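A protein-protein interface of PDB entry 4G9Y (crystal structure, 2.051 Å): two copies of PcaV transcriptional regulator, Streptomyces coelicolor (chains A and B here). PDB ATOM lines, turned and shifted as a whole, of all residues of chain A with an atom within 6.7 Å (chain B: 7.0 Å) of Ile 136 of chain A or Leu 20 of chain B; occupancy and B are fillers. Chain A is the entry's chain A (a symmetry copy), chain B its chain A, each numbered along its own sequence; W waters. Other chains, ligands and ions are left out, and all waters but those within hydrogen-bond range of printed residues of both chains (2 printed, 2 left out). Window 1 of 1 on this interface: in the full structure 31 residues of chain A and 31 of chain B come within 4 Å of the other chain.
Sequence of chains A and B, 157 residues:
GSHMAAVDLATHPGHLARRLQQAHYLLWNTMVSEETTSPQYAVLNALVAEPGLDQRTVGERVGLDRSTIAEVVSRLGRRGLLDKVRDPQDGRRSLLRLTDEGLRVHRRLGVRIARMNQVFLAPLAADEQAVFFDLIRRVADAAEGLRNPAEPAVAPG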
ATOM      1  N   PRO A  13      26.269   8.041  -5.445  1.00  0.00           N
ATOM      2  CA  PRO A  13      25.844   8.339  -6.811  1.00  0.00           C
ATOM      3  C   PRO A  13      24.322   8.391  -6.962  1.00  0.00           C
ATOM      4  O   PRO A  13      23.866   8.973  -7.913  1.00  0.00           O
ATOM      5  CB  PRO A  13      26.426   7.179  -7.618  1.00  0.00           C
ATOM      6  CG  PRO A  13      26.545   6.055  -6.621  1.00  0.00           C
ATOM      7  CD  PRO A  13      26.861   6.695  -5.311  1.00  0.00           C
ATOM      8  N   LEU A  16      23.493  11.982  -6.332  1.00  0.00           N
ATOM      9  CA  LEU A  16      23.958  12.787  -7.441  1.00  0.00           C
ATOM     10  C   LEU A  16      23.036  12.649  -8.643  1.00  0.00           C
ATOM     11  O   LEU A  16      22.749  13.633  -9.323  1.00  0.00           O
ATOM     12  CB  LEU A  16      25.385  12.387  -7.828  1.00  0.00           C
ATOM     13  CG  LEU A  16      26.087  13.396  -8.737  1.00  0.00           C
ATOM     14  CD1 LEU A  16      26.272  14.745  -8.039  1.00  0.00           C
ATOM     15  CD2 LEU A  16      27.404  12.862  -9.256  1.00  0.00           C
ATOM     16  N   ALA A  17      22.556  11.442  -8.916  1.00  0.00           N
ATOM     17  CA  ALA A  17      21.667  11.266 -10.080  1.00  0.00           C
ATOM     18  C   ALA A  17      20.357  12.019  -9.909  1.00  0.00           C
ATOM     19  O   ALA A  17      19.866  12.629 -10.845  1.00  0.00           O
ATOM     20  CB  ALA A  17      21.389   9.786 -10.354  1.00  0.00           C
ATOM     21  N   ARG A  18      19.793  11.976  -8.707  1.00  0.00           N
ATOM     22  CA  ARG A  18      18.571  12.716  -8.432  1.00  0.00           C
ATOM     23  C   ARG A  18      18.801  14.230  -8.576  1.00  0.00           C
ATOM     24  O   ARG A  18      17.962  14.925  -9.129  1.00  0.00           O
ATOM     25  CB  ARG A  18      18.004  12.351  -7.044  1.00  0.00           C
ATOM     26  CG  ARG A  18      17.540  10.884  -6.947  1.00  0.00           C
ATOM     27  CD  ARG A  18      16.758  10.553  -5.660  1.00  0.00           C
ATOM     28  NE  ARG A  18      17.604  10.572  -4.463  1.00  0.00           N
ATOM     29  CZ  ARG A  18      18.302   9.533  -4.006  1.00  0.00           C
ATOM     30  NH1 ARG A  18      18.272   8.359  -4.635  1.00  0.00           N
ATOM     31  NH2 ARG A  18      19.040   9.668  -2.912  1.00  0.00           N
ATOM     32  N   LEU A  20      20.937  15.749 -10.561  1.00  0.00           N
ATOM     33  CA  LEU A  20      21.080  16.065 -11.975  1.00  0.00           C
ATOM     34  C   LEU A  20      19.722  16.136 -12.631  1.00  0.00           C
ATOM     35  O   LEU A  20      19.438  17.026 -13.429  1.00  0.00           O
ATOM     36  CB  LEU A  20      21.915  14.994 -12.683  1.00  0.00           C
ATOM     37  CG  LEU A  20      22.135  15.241 -14.179  1.00  0.00           C
ATOM     38  CD1 LEU A  20      22.961  16.509 -14.400  1.00  0.00           C
ATOM     39  CD2 LEU A  20      22.824  14.041 -14.812  1.00  0.00           C
ATOM     40  N   VAL A 131      32.140  13.275 -23.225  1.00  0.00           N
ATOM     41  CA  VAL A 131      32.462  12.350 -22.133  1.00  0.00           C
ATOM     42  C   VAL A 131      31.272  12.171 -21.179  1.00  0.00           C
ATOM     43  O   VAL A 131      30.944  11.040 -20.785  1.00  0.00           O
ATOM     44  CB  VAL A 131      33.740  12.788 -21.374  1.00  0.00           C
ATOM     45  CG1 VAL A 131      33.878  12.048 -20.043  1.00  0.00           C
ATOM     46  CG2 VAL A 131      34.967  12.524 -22.240  1.00  0.00           C
ATOM     47  N   PHE A 132      30.601  13.283 -20.860  1.00  0.00           N
ATOM     48  CA  PHE A 132      29.408  13.293 -19.995  1.00  0.00           C
ATOM     49  C   PHE A 132      28.386  12.296 -20.539  1.00  0.00           C
ATOM     50  O   PHE A 132      27.879  11.443 -19.812  1.00  0.00           O
ATOM     51  CB  PHE A 132      28.862  14.729 -19.958  1.00  0.00           C
ATOM     52  CG  PHE A 132      27.539  14.914 -19.248  1.00  0.00           C
ATOM     53  CD1 PHE A 132      27.496  15.246 -17.903  1.00  0.00           C
ATOM     54  CD2 PHE A 132      26.347  14.869 -19.955  1.00  0.00           C
ATOM     55  CE1 PHE A 132      26.281  15.492 -17.262  1.00  0.00           C
ATOM     56  CE2 PHE A 132      25.125  15.087 -19.329  1.00  0.00           C
ATOM     57  CZ  PHE A 132      25.089  15.414 -17.969  1.00  0.00           C
ATOM     58  N   PHE A 133      28.102  12.370 -21.830  1.00  0.00           N
ATOM     59  CA  PHE A 133      27.138  11.427 -22.422  1.00  0.00           C
ATOM     60  C   PHE A 133      27.630   9.985 -22.404  1.00  0.00           C
ATOM     61  O   PHE A 133      26.881   9.066 -22.069  1.00  0.00           O
ATOM     62  CB  PHE A 133      26.764  11.836 -23.847  1.00  0.00           C
ATOM     63  CG  PHE A 133      25.734  12.900 -23.892  1.00  0.00           C
ATOM     64  CD1 PHE A 133      24.384  12.574 -23.835  1.00  0.00           C
ATOM     65  CD2 PHE A 133      26.100  14.227 -23.938  1.00  0.00           C
ATOM     66  CE1 PHE A 133      23.413  13.567 -23.837  1.00  0.00           C
ATOM     67  CE2 PHE A 133      25.142  15.228 -23.936  1.00  0.00           C
ATOM     68  CZ  PHE A 133      23.796  14.901 -23.881  1.00  0.00           C
ATOM     69  N   ASP A 134      28.886   9.791 -22.780  1.00  0.00           N
ATOM     70  CA  ASP A 134      29.462   8.452 -22.821  1.00  0.00           C
ATOM     71  C   ASP A 134      29.390   7.776 -21.466  1.00  0.00           C
ATOM     72  O   ASP A 134      28.915   6.644 -21.368  1.00  0.00           O
ATOM     73  CB  ASP A 134      30.921   8.471 -23.287  1.00  0.00           C
ATOM     74  CG  ASP A 134      31.530   7.057 -23.344  1.00  0.00           C
ATOM     75  OD1 ASP A 134      30.982   6.202 -24.069  1.00  0.00           O
ATOM     76  OD2 ASP A 134      32.541   6.793 -22.652  1.00  0.00           O
ATOM     77  N   LEU A 135      29.843   8.468 -20.422  1.00  0.00           N
ATOM     78  CA  LEU A 135      29.890   7.870 -19.094  1.00  0.00           C
ATOM     79  C   LEU A 135      28.498   7.571 -18.545  1.00  0.00           C
ATOM     80  O   LEU A 135      28.266   6.509 -17.973  1.00  0.00           O
ATOM     81  CB  LEU A 135      30.641   8.769 -18.107  1.00  0.00           C
ATOM     82  CG  LEU A 135      32.086   9.089 -18.469  1.00  0.00           C
ATOM     83  CD1 LEU A 135      32.729   9.942 -17.366  1.00  0.00           C
ATOM     84  CD2 LEU A 135      32.892   7.824 -18.782  1.00  0.00           C
ATOM     85  N   ILE A 136      27.577   8.521 -18.685  1.00  0.00           N
ATOM     86  CA  ILE A 136      26.246   8.316 -18.150  1.00  0.00           C
ATOM     87  C   ILE A 136      25.541   7.179 -18.904  1.00  0.00           C
ATOM     88  O   ILE A 136      24.883   6.321 -18.300  1.00  0.00           O
ATOM     89  CB  ILE A 136      25.432   9.626 -18.186  1.00  0.00           C
ATOM     90  CG1 ILE A 136      26.054  10.635 -17.218  1.00  0.00           C
ATOM     91  CG2 ILE A 136      23.985   9.372 -17.798  1.00  0.00           C
ATOM     92  CD1 ILE A 136      25.405  12.036 -17.284  1.00  0.00           C
ATOM     93  N   ARG A 137      25.700   7.146 -20.225  1.00  0.00           N
ATOM     94  CA  ARG A 137      25.105   6.044 -20.991  1.00  0.00           C
ATOM     95  C   ARG A 137      25.645   4.692 -20.582  1.00  0.00           C
ATOM     96  O   ARG A 137      24.884   3.742 -20.470  1.00  0.00           O
ATOM     97  CB  ARG A 137      25.304   6.217 -22.488  1.00  0.00           C
ATOM     98  CG  ARG A 137      24.383   7.227 -23.075  1.00  0.00           C
ATOM     99  CD  ARG A 137      24.523   7.233 -24.586  1.00  0.00           C
ATOM    100  NE  ARG A 137      23.683   8.270 -25.160  1.00  0.00           N
ATOM    101  CZ  ARG A 137      24.110   9.136 -26.064  1.00  0.00           C
ATOM    102  NH1 ARG A 137      25.364   9.063 -26.491  1.00  0.00           N
ATOM    103  NH2 ARG A 137      23.287  10.057 -26.543  1.00  0.00           N
ATOM    104  N   ARG A 138      26.956   4.594 -20.369  1.00  0.00           N
ATOM    105  CA  ARG A 138      27.540   3.319 -19.964  1.00  0.00           C
ATOM    106  C   ARG A 138      26.981   2.871 -18.622  1.00  0.00           C
ATOM    107  O   ARG A 138      26.684   1.695 -18.430  1.00  0.00           O
ATOM    108  CB  ARG A 138      29.071   3.396 -19.927  1.00  0.00           C
ATOM    109  CG  ARG A 138      29.713   3.303 -21.329  1.00  0.00           C
ATOM    110  CD  ARG A 138      31.157   3.820 -21.333  1.00  0.00           C
ATOM    111  NE  ARG A 138      32.006   3.136 -20.356  1.00  0.00           N
ATOM    112  CZ  ARG A 138      33.219   3.553 -20.004  1.00  0.00           C
ATOM    113  NH1 ARG A 138      33.736   4.646 -20.550  1.00  0.00           N
ATOM    114  NH2 ARG A 138      33.927   2.870 -19.118  1.00  0.00           N
ATOM    115  N   VAL A 139      26.822   3.811 -17.695  1.00  0.00           N
ATOM    116  CA  VAL A 139      26.309   3.482 -16.365  1.00  0.00           C
ATOM    117  C   VAL A 139      24.837   3.075 -16.441  1.00  0.00           C
ATOM    118  O   VAL A 139      24.431   2.061 -15.864  1.00  0.00           O
ATOM    119  CB  VAL A 139      26.502   4.673 -15.375  1.00  0.00           C
ATOM    120  CG1 VAL A 139      25.733   4.437 -14.071  1.00  0.00           C
ATOM    121  CG2 VAL A 139      27.984   4.864 -15.089  1.00  0.00           C
ATOM    122  N   ALA A 140      24.027   3.850 -17.153  1.00  0.00           N
ATOM    123  CA  ALA A 140      22.610   3.515 -17.234  1.00  0.00           C
ATOM    124  C   ALA A 140      22.395   2.194 -17.987  1.00  0.00           C
ATOM    125  O   ALA A 140      21.543   1.383 -17.604  1.00  0.00           O
ATOM    126  CB  ALA A 140      21.803   4.649 -17.889  1.00  0.00           C
ATOM    127  N   ASP A 141      23.168   1.975 -19.051  1.00  0.00           N
ATOM    128  CA  ASP A 141      22.960   0.795 -19.901  1.00  0.00           C
ATOM    129  C   ASP A 141      23.296  -0.456 -19.109  1.00  0.00           C
ATOM    130  O   ASP A 141      22.585  -1.455 -19.186  1.00  0.00           O
ATOM    131  CB  ASP A 141      23.818   0.820 -21.185  1.00  0.00           C
ATOM    132  CG  ASP A 141      23.373   1.887 -22.201  1.00  0.00           C
ATOM    133  OD1 ASP A 141      22.328   2.556 -21.998  1.00  0.00           O
ATOM    134  OD2 ASP A 141      24.088   2.044 -23.224  1.00  0.00           O
ATOM    135  N   GLU A 144      20.635  -1.269 -16.438  1.00  0.00           N
ATOM    136  CA  GLU A 144      19.393  -1.765 -17.016  1.00  0.00           C
ATOM    137  C   GLU A 144      19.585  -3.096 -17.749  1.00  0.00           C
ATOM    138  O   GLU A 144      18.619  -3.723 -18.177  1.00  0.00           O
ATOM    139  CB  GLU A 144      18.768  -0.704 -17.922  1.00  0.00           C
ATOM    140  CG  GLU A 144      18.284   0.503 -17.139  1.00  0.00           C
ATOM    141  CD  GLU A 144      17.926   1.692 -18.024  1.00  0.00           C
ATOM    142  OE1 GLU A 144      18.091   1.584 -19.262  1.00  0.00           O
ATOM    143  OE2 GLU A 144      17.486   2.731 -17.471  1.00  0.00           O
ATOM    144  N   PRO B  13      19.823  15.777 -23.043  1.00  0.00           N
ATOM    145  CA  PRO B  13      20.360  15.483 -21.715  1.00  0.00           C
ATOM    146  C   PRO B  13      19.268  15.323 -20.655  1.00  0.00           C
ATOM    147  O   PRO B  13      19.545  14.733 -19.641  1.00  0.00           O
ATOM    148  CB  PRO B  13      21.228  16.705 -21.413  1.00  0.00           C
ATOM    149  CG  PRO B  13      20.620  17.808 -22.239  1.00  0.00           C
ATOM    150  CD  PRO B  13      20.103  17.159 -23.480  1.00  0.00           C
ATOM    151  N   HIS B  15      16.419  13.599 -21.012  1.00  0.00           N
ATOM    152  CA  HIS B  15      16.164  12.171 -21.164  1.00  0.00           C
ATOM    153  C   HIS B  15      17.239  11.331 -20.472  1.00  0.00           C
ATOM    154  O   HIS B  15      16.938  10.421 -19.711  1.00  0.00           O
ATOM    155  CB  HIS B  15      16.099  11.829 -22.652  1.00  0.00           C
ATOM    156  CG  HIS B  15      16.106  10.360 -22.948  1.00  0.00           C
ATOM    157  ND1 HIS B  15      14.985   9.565 -22.818  1.00  0.00           N
ATOM    158  CD2 HIS B  15      17.097   9.544 -23.386  1.00  0.00           C
ATOM    159  CE1 HIS B  15      15.289   8.323 -23.155  1.00  0.00           C
ATOM    160  NE2 HIS B  15      16.564   8.282 -23.503  1.00  0.00           N
ATOM    161  N   LEU B  16      18.498  11.665 -20.729  1.00  0.00           N
ATOM    162  CA  LEU B  16      19.608  10.926 -20.169  1.00  0.00           C
ATOM    163  C   LEU B  16      19.623  11.025 -18.651  1.00  0.00           C
ATOM    164  O   LEU B  16      19.893  10.041 -17.965  1.00  0.00           O
ATOM    165  CB  LEU B  16      20.933  11.441 -20.739  1.00  0.00           C
ATOM    166  CG  LEU B  16      22.120  10.511 -20.486  1.00  0.00           C
ATOM    167  CD1 LEU B  16      21.932   9.161 -21.184  1.00  0.00           C
ATOM    168  CD2 LEU B  16      23.431  11.155 -20.882  1.00  0.00           C
ATOM    169  N   ALA B  17      19.327  12.200 -18.109  1.00  0.00           N
ATOM    170  CA  ALA B  17      19.340  12.340 -16.640  1.00  0.00           C
ATOM    171  C   ALA B  17      18.267  11.487 -15.981  1.00  0.00           C
ATOM    172  O   ALA B  17      18.508  10.867 -14.959  1.00  0.00           O
ATOM    173  CB  ALA B  17      19.183  13.801 -16.213  1.00  0.00           C
ATOM    174  N   ARG B  18      17.078  11.457 -16.574  1.00  0.00           N
ATOM    175  CA  ARG B  18      16.008  10.621 -16.050  1.00  0.00           C
ATOM    176  C   ARG B  18      16.390   9.132 -16.119  1.00  0.00           C
ATOM    177  O   ARG B  18      16.129   8.391 -15.183  1.00  0.00           O
ATOM    178  CB  ARG B  18      14.678  10.905 -16.778  1.00  0.00           C
ATOM    179  CG  ARG B  18      14.146  12.331 -16.529  1.00  0.00           C
ATOM    180  CD  ARG B  18      12.713  12.570 -17.046  1.00  0.00           C
ATOM    181  NE  ARG B  18      12.633  12.582 -18.509  1.00  0.00           N
ATOM    182  CZ  ARG B  18      12.817  13.659 -19.274  1.00  0.00           C
ATOM    183  NH1 ARG B  18      13.097  14.844 -18.732  1.00  0.00           N
ATOM    184  NH2 ARG B  18      12.727  13.551 -20.592  1.00  0.00           N
ATOM    185  N   ARG B  19      17.002   8.705 -17.222  1.00  0.00           N
ATOM    186  CA  ARG B  19      17.490   7.322 -17.341  1.00  0.00           C
ATOM    187  C   ARG B  19      18.457   6.942 -16.223  1.00  0.00           C
ATOM    188  O   ARG B  19      18.374   5.852 -15.674  1.00  0.00           O
ATOM    189  CB  ARG B  19      18.233   7.099 -18.665  1.00  0.00           C
ATOM    190  CG  ARG B  19      17.385   6.860 -19.878  1.00  0.00           C
ATOM    191  CD  ARG B  19      18.247   6.270 -21.002  1.00  0.00           C
ATOM    192  NE  ARG B  19      18.594   4.884 -20.707  1.00  0.00           N
ATOM    193  CZ  ARG B  19      19.726   4.288 -21.063  1.00  0.00           C
ATOM    194  NH1 ARG B  19      20.673   4.953 -21.733  1.00  0.00           N
ATOM    195  NH2 ARG B  19      19.919   3.016 -20.736  1.00  0.00           N
ATOM    196  N   LEU B  20      19.402   7.829 -15.925  1.00  0.00           N
ATOM    197  CA  LEU B  20      20.413   7.561 -14.912  1.00  0.00           C
ATOM    198  C   LEU B  20      19.764   7.405 -13.559  1.00  0.00           C
ATOM    199  O   LEU B  20      20.103   6.518 -12.780  1.00  0.00           O
ATOM    200  CB  LEU B  20      21.425   8.710 -14.849  1.00  0.00           C
ATOM    201  CG  LEU B  20      22.542   8.517 -13.817  1.00  0.00           C
ATOM    202  CD1 LEU B  20      23.419   7.320 -14.188  1.00  0.00           C
ATOM    203  CD2 LEU B  20      23.383   9.782 -13.716  1.00  0.00           C
ATOM    204  N   GLN B  21      18.820   8.283 -13.262  1.00  0.00           N
ATOM    205  CA  GLN B  21      18.134   8.187 -11.986  1.00  0.00           C
ATOM    206  C   GLN B  21      17.278   6.922 -11.914  1.00  0.00           C
ATOM    207  O   GLN B  21      17.256   6.236 -10.899  1.00  0.00           O
ATOM    208  CB  GLN B  21      17.275   9.439 -11.761  1.00  0.00           C
ATOM    209  CG  GLN B  21      16.728   9.549 -10.349  1.00  0.00           C
ATOM    210  CD  GLN B  21      15.422   8.804 -10.171  1.00  0.00           C
ATOM    211  OE1 GLN B  21      14.674   8.596 -11.133  1.00  0.00           O
ATOM    212  NE2 GLN B  21      15.134   8.399  -8.935  1.00  0.00           N
ATOM    213  N   GLN B  22      16.572   6.610 -12.996  1.00  0.00           N
ATOM    214  CA  GLN B  22      15.769   5.392 -13.046  1.00  0.00           C
ATOM    215  C   GLN B  22      16.613   4.126 -12.941  1.00  0.00           C
ATOM    216  O   GLN B  22      16.200   3.146 -12.329  1.00  0.00           O
ATOM    217  CB  GLN B  22      14.951   5.355 -14.336  1.00  0.00           C
ATOM    218  CG  GLN B  22      13.872   6.425 -14.361  1.00  0.00           C
ATOM    219  CD  GLN B  22      13.045   6.420 -15.640  1.00  0.00           C
ATOM    220  OE1 GLN B  22      13.258   5.595 -16.539  1.00  0.00           O
ATOM    221  NE2 GLN B  22      12.087   7.342 -15.724  1.00  0.00           N
ATOM    222  N   ALA B  23      17.786   4.143 -13.560  1.00  0.00           N
ATOM    223  CA  ALA B  23      18.692   3.008 -13.463  1.00  0.00           C
ATOM    224  C   ALA B  23      19.125   2.783 -12.015  1.00  0.00           C
ATOM    225  O   ALA B  23      19.229   1.648 -11.565  1.00  0.00           O
ATOM    226  CB  ALA B  23      19.906   3.228 -14.363  1.00  0.00           C
ATOM    227  N   HIS B  24      19.366   3.857 -11.272  1.00  0.00           N
ATOM    228  CA  HIS B  24      19.744   3.694  -9.867  1.00  0.00           C
ATOM    229  C   HIS B  24      18.568   3.144  -9.045  1.00  0.00           C
ATOM    230  O   HIS B  24      18.739   2.286  -8.175  1.00  0.00           O
ATOM    231  CB  HIS B  24      20.227   5.019  -9.275  1.00  0.00           C
ATOM    232  CG  HIS B  24      20.833   4.867  -7.920  1.00  0.00           C
ATOM    233  ND1 HIS B  24      20.088   4.923  -6.764  1.00  0.00           N
ATOM    234  CD2 HIS B  24      22.105   4.608  -7.538  1.00  0.00           C
ATOM    235  CE1 HIS B  24      20.880   4.720  -5.725  1.00  0.00           C
ATOM    236  NE2 HIS B  24      22.109   4.532  -6.168  1.00  0.00           N
ATOM    237  N   TYR B  25      17.369   3.638  -9.335  1.00  0.00           N
ATOM    238  CA  TYR B  25      16.156   3.166  -8.661  1.00  0.00           C
ATOM    239  C   TYR B  25      15.931   1.683  -8.945  1.00  0.00           C
ATOM    240  O   TYR B  25      15.562   0.916  -8.050  1.00  0.00           O
ATOM    241  CB  TYR B  25      14.946   3.995  -9.122  1.00  0.00           C
ATOM    242  CG  TYR B  25      13.615   3.572  -8.537  1.00  0.00           C
ATOM    243  CD1 TYR B  25      12.754   2.741  -9.243  1.00  0.00           C
ATOM    244  CD2 TYR B  25      13.214   4.020  -7.279  1.00  0.00           C
ATOM    245  CE1 TYR B  25      11.529   2.362  -8.707  1.00  0.00           C
ATOM    246  CE2 TYR B  25      12.001   3.651  -6.739  1.00  0.00           C
ATOM    247  CZ  TYR B  25      11.162   2.820  -7.454  1.00  0.00           C
ATOM    248  OH  TYR B  25       9.952   2.453  -6.915  1.00  0.00           O
ATOM    249  N   PHE B 120      26.785  -0.150  -9.419  1.00  0.00           N
ATOM    250  CA  PHE B 120      26.290   0.959 -10.244  1.00  0.00           C
ATOM    251  C   PHE B 120      27.401   1.709 -11.011  1.00  0.00           C
ATOM    252  O   PHE B 120      27.241   2.057 -12.194  1.00  0.00           O
ATOM    253  CB  PHE B 120      25.518   1.938  -9.342  1.00  0.00           C
ATOM    254  CG  PHE B 120      24.820   3.054 -10.076  1.00  0.00           C
ATOM    255  CD1 PHE B 120      23.763   2.788 -10.929  1.00  0.00           C
ATOM    256  CD2 PHE B 120      25.190   4.373  -9.865  1.00  0.00           C
ATOM    257  CE1 PHE B 120      23.090   3.822 -11.576  1.00  0.00           C
ATOM    258  CE2 PHE B 120      24.530   5.425 -10.519  1.00  0.00           C
ATOM    259  CZ  PHE B 120      23.472   5.148 -11.371  1.00  0.00           C
ATOM    260  N   LEU B 124      32.656   1.882 -15.061  1.00  0.00           N
ATOM    261  CA  LEU B 124      33.663   2.929 -15.182  1.00  0.00           C
ATOM    262  C   LEU B 124      34.947   2.554 -14.436  1.00  0.00           C
ATOM    263  O   LEU B 124      34.896   2.062 -13.301  1.00  0.00           O
ATOM    264  CB  LEU B 124      33.112   4.223 -14.597  1.00  0.00           C
ATOM    265  CG  LEU B 124      31.759   4.675 -15.167  1.00  0.00           C
ATOM    266  CD1 LEU B 124      31.444   6.062 -14.630  1.00  0.00           C
ATOM    267  CD2 LEU B 124      31.726   4.675 -16.700  1.00  0.00           C
ATOM    268  N   PHE B 132      33.151  11.275 -13.771  1.00  0.00           N
ATOM    269  CA  PHE B 132      31.684  11.152 -13.712  1.00  0.00           C
ATOM    270  C   PHE B 132      31.149  12.084 -12.625  1.00  0.00           C
ATOM    271  O   PHE B 132      30.238  12.877 -12.859  1.00  0.00           O
ATOM    272  CB  PHE B 132      31.341   9.679 -13.438  1.00  0.00           C
ATOM    273  CG  PHE B 132      29.882   9.378 -13.180  1.00  0.00           C
ATOM    274  CD1 PHE B 132      29.038   9.008 -14.218  1.00  0.00           C
ATOM    275  CD2 PHE B 132      29.385   9.352 -11.886  1.00  0.00           C
ATOM    276  CE1 PHE B 132      27.711   8.656 -13.973  1.00  0.00           C
ATOM    277  CE2 PHE B 132      28.059   9.028 -11.625  1.00  0.00           C
ATOM    278  CZ  PHE B 132      27.212   8.665 -12.678  1.00  0.00           C
ATOM    279  N   LEU B 135      31.929  16.006 -13.521  1.00  0.00           N
ATOM    280  CA  LEU B 135      31.098  16.571 -14.576  1.00  0.00           C
ATOM    281  C   LEU B 135      29.648  16.751 -14.137  1.00  0.00           C
ATOM    282  O   LEU B 135      29.033  17.777 -14.414  1.00  0.00           O
ATOM    283  CB  LEU B 135      31.140  15.705 -15.839  1.00  0.00           C
ATOM    284  CG  LEU B 135      32.517  15.504 -16.458  1.00  0.00           C
ATOM    285  CD1 LEU B 135      32.400  14.672 -17.745  1.00  0.00           C
ATOM    286  CD2 LEU B 135      33.247  16.833 -16.680  1.00  0.00           C
ATOM    287  N   ILE B 136      29.085  15.739 -13.481  1.00  0.00           N
ATOM    288  CA  ILE B 136      27.698  15.831 -13.070  1.00  0.00           C
ATOM    289  C   ILE B 136      27.531  16.931 -12.012  1.00  0.00           C
ATOM    290  O   ILE B 136      26.579  17.722 -12.056  1.00  0.00           O
ATOM    291  CB  ILE B 136      27.183  14.465 -12.572  1.00  0.00           C
ATOM    292  CG1 ILE B 136      27.145  13.481 -13.742  1.00  0.00           C
ATOM    293  CG2 ILE B 136      25.793  14.602 -11.972  1.00  0.00           C
ATOM    294  CD1 ILE B 136      26.782  12.037 -13.325  1.00  0.00           C
HETATM  295  O   HOH W   1      20.344  11.796 -13.304  1.00  0.00           O
HETATM  296  O   HOH W   2      25.734   0.556 -13.877  1.00  0.00           O
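Leu 16 of chain A touches Ile 136 of chain B, and with the chains exchanged Ile 136 of chain A touches Leu 16 of chain B.
Ala 17 of chain A touches Leu 20 of chain B, and with the chains exchanged Leu 20 of chain A touches Ala 17 of chain B.
Leu 20 of chain A touches Ile 136 of chain B, and with the chains exchanged Ile 136 of chain A touches Leu 20 of chain B.
Phe 132 of chain A touches Leu 135 of chain B, and with the chains exchanged Leu 135 of chain A touches Phe 132 of chain B.
Of the 17 printed residues of chain B, 12 touch a printed residue of chain A.
Hydrophobic or aromatic side chains of chain B within 4 Å of the printed part of chain A: Pro 13, Leu 16, Ala 17, Leu 20, Ala 23, Phe 120, Leu 124, Phe 132, Leu 135 and Ile 136.
Of the 17 printed residues of chain A, 16 touch a printed residue of chain B.
Among the printed residues, 26 pairs touch across the chains.
Of the printed residues of chain B, Ile 136 of chain A touches Leu 16 (3.5 Å) and Leu 20 (3.96 Å).
Leu 20 of chain B touches three residues of chain A.
Of the printed residues of chain A, Pro 13 of chain B touches Phe 133 (3.99 Å).
Of the printed residues of chain B, Ala 140 of chain A touches Arg 19 (3.8 Å) and Ala 23 (3.95 Å).
Of the printed residues of chain B, Asp 141 of chain A touches Arg 19 (2.8 Å).
Of the printed residues of chain A, Phe 132 of chain B touches Leu 135 and Val 139.
The nearest residue of chain B that does not touch Ile 136 of chain A is Phe 132 of chain B (4.1 Å).
The nearest residue of chain A that does not touch Leu 20 of chain B is Ala 140 of chain A (4.4 Å).
The nearest printed residue of chain A that does not touch Ala 23 of chain B is Val 139 of chain A (4.9 Å).
OD2 of Asp 134 of chain A is in salt-bridge range of NH1 of Arg 138 of chain A (3.2 Å).
Water W1 lies within hydrogen-bond range of the backbone carbonyl oxygen (O) of Ala 17 of chain B (2.6 Å) and the backbone carbonyl oxygen (O) of Ala 17 of chain A (2.6 Å).
Water W2 lies within hydrogen-bond range of O of Phe 120 of chain B (2.7 Å) and O of Val 139 of chain A (2.8 Å).
Among the printed residues, merely in contact across the chains: Pro 13 of chain A with Phe 120 of chain B (3.8 Å), Leu 16 of chain A with Ile 136 of chain B (3.5 Å), Ala 17 of chain A with Leu 20 of chain B (3.9 Å), Ala 17 of chain A with Gln 21 of chain B (3.98 Å), Arg 18 of chain A with Gln 21 of chain B (3.7 Å), Leu 20 of chain A with Ala 17 of chain B (3.9 Å), Leu 20 of chain A with Ile 136 of chain B (3.96 Å), Val 131 of chain A with Leu 135 of chain B (3.8 Å), Phe 132 of chain A with Leu 135 of chain B (3.9 Å), Phe 133 of chain A with Pro 13 of chain B (3.99 Å), Phe 133 of chain A with Leu 16 of chain B (3.4 Å), Leu 135 of chain A with Leu 124 of chain B (3.95 Å), Leu 135 of chain A with Phe 132 of chain B (3.9 Å), Ile 136 of chain A with Leu 16 of chain B (3.5 Å), Ile 136 of chain A with Leu 20 of chain B (3.96 Å), Arg 137 of chain A with Leu 16 of chain B (3.7 Å), Arg 138 of chain A with Leu 124 of chain B (3.7 Å), Val 139 of chain A with Leu 20 of chain B (3.7 Å), Val 139 of chain A with Phe 120 of chain B (3.4 Å), Val 139 of chain A with Leu 124 of chain B (3.7 Å), Val 139 of chain A with Phe 132 of chain B (3.96 Å), Ala 140 of chain A with Arg 19 of chain B (3.8 Å), Ala 140 of chain A with Ala 23 of chain B (3.95 Å) and Glu 144 of chain A with Ala 23 of chain B (3.97 Å).
OD1 of Asp 141 of chain A is in salt-bridge range of NH2 of Arg 19 of chain B, at 2.8 Å.
The guanidinium group (NH2) of Arg 19 of chain B lies within salt-bridge range of the side-chain carboxylate (OE1) of Glu 144 of chain A (2.8 Å).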
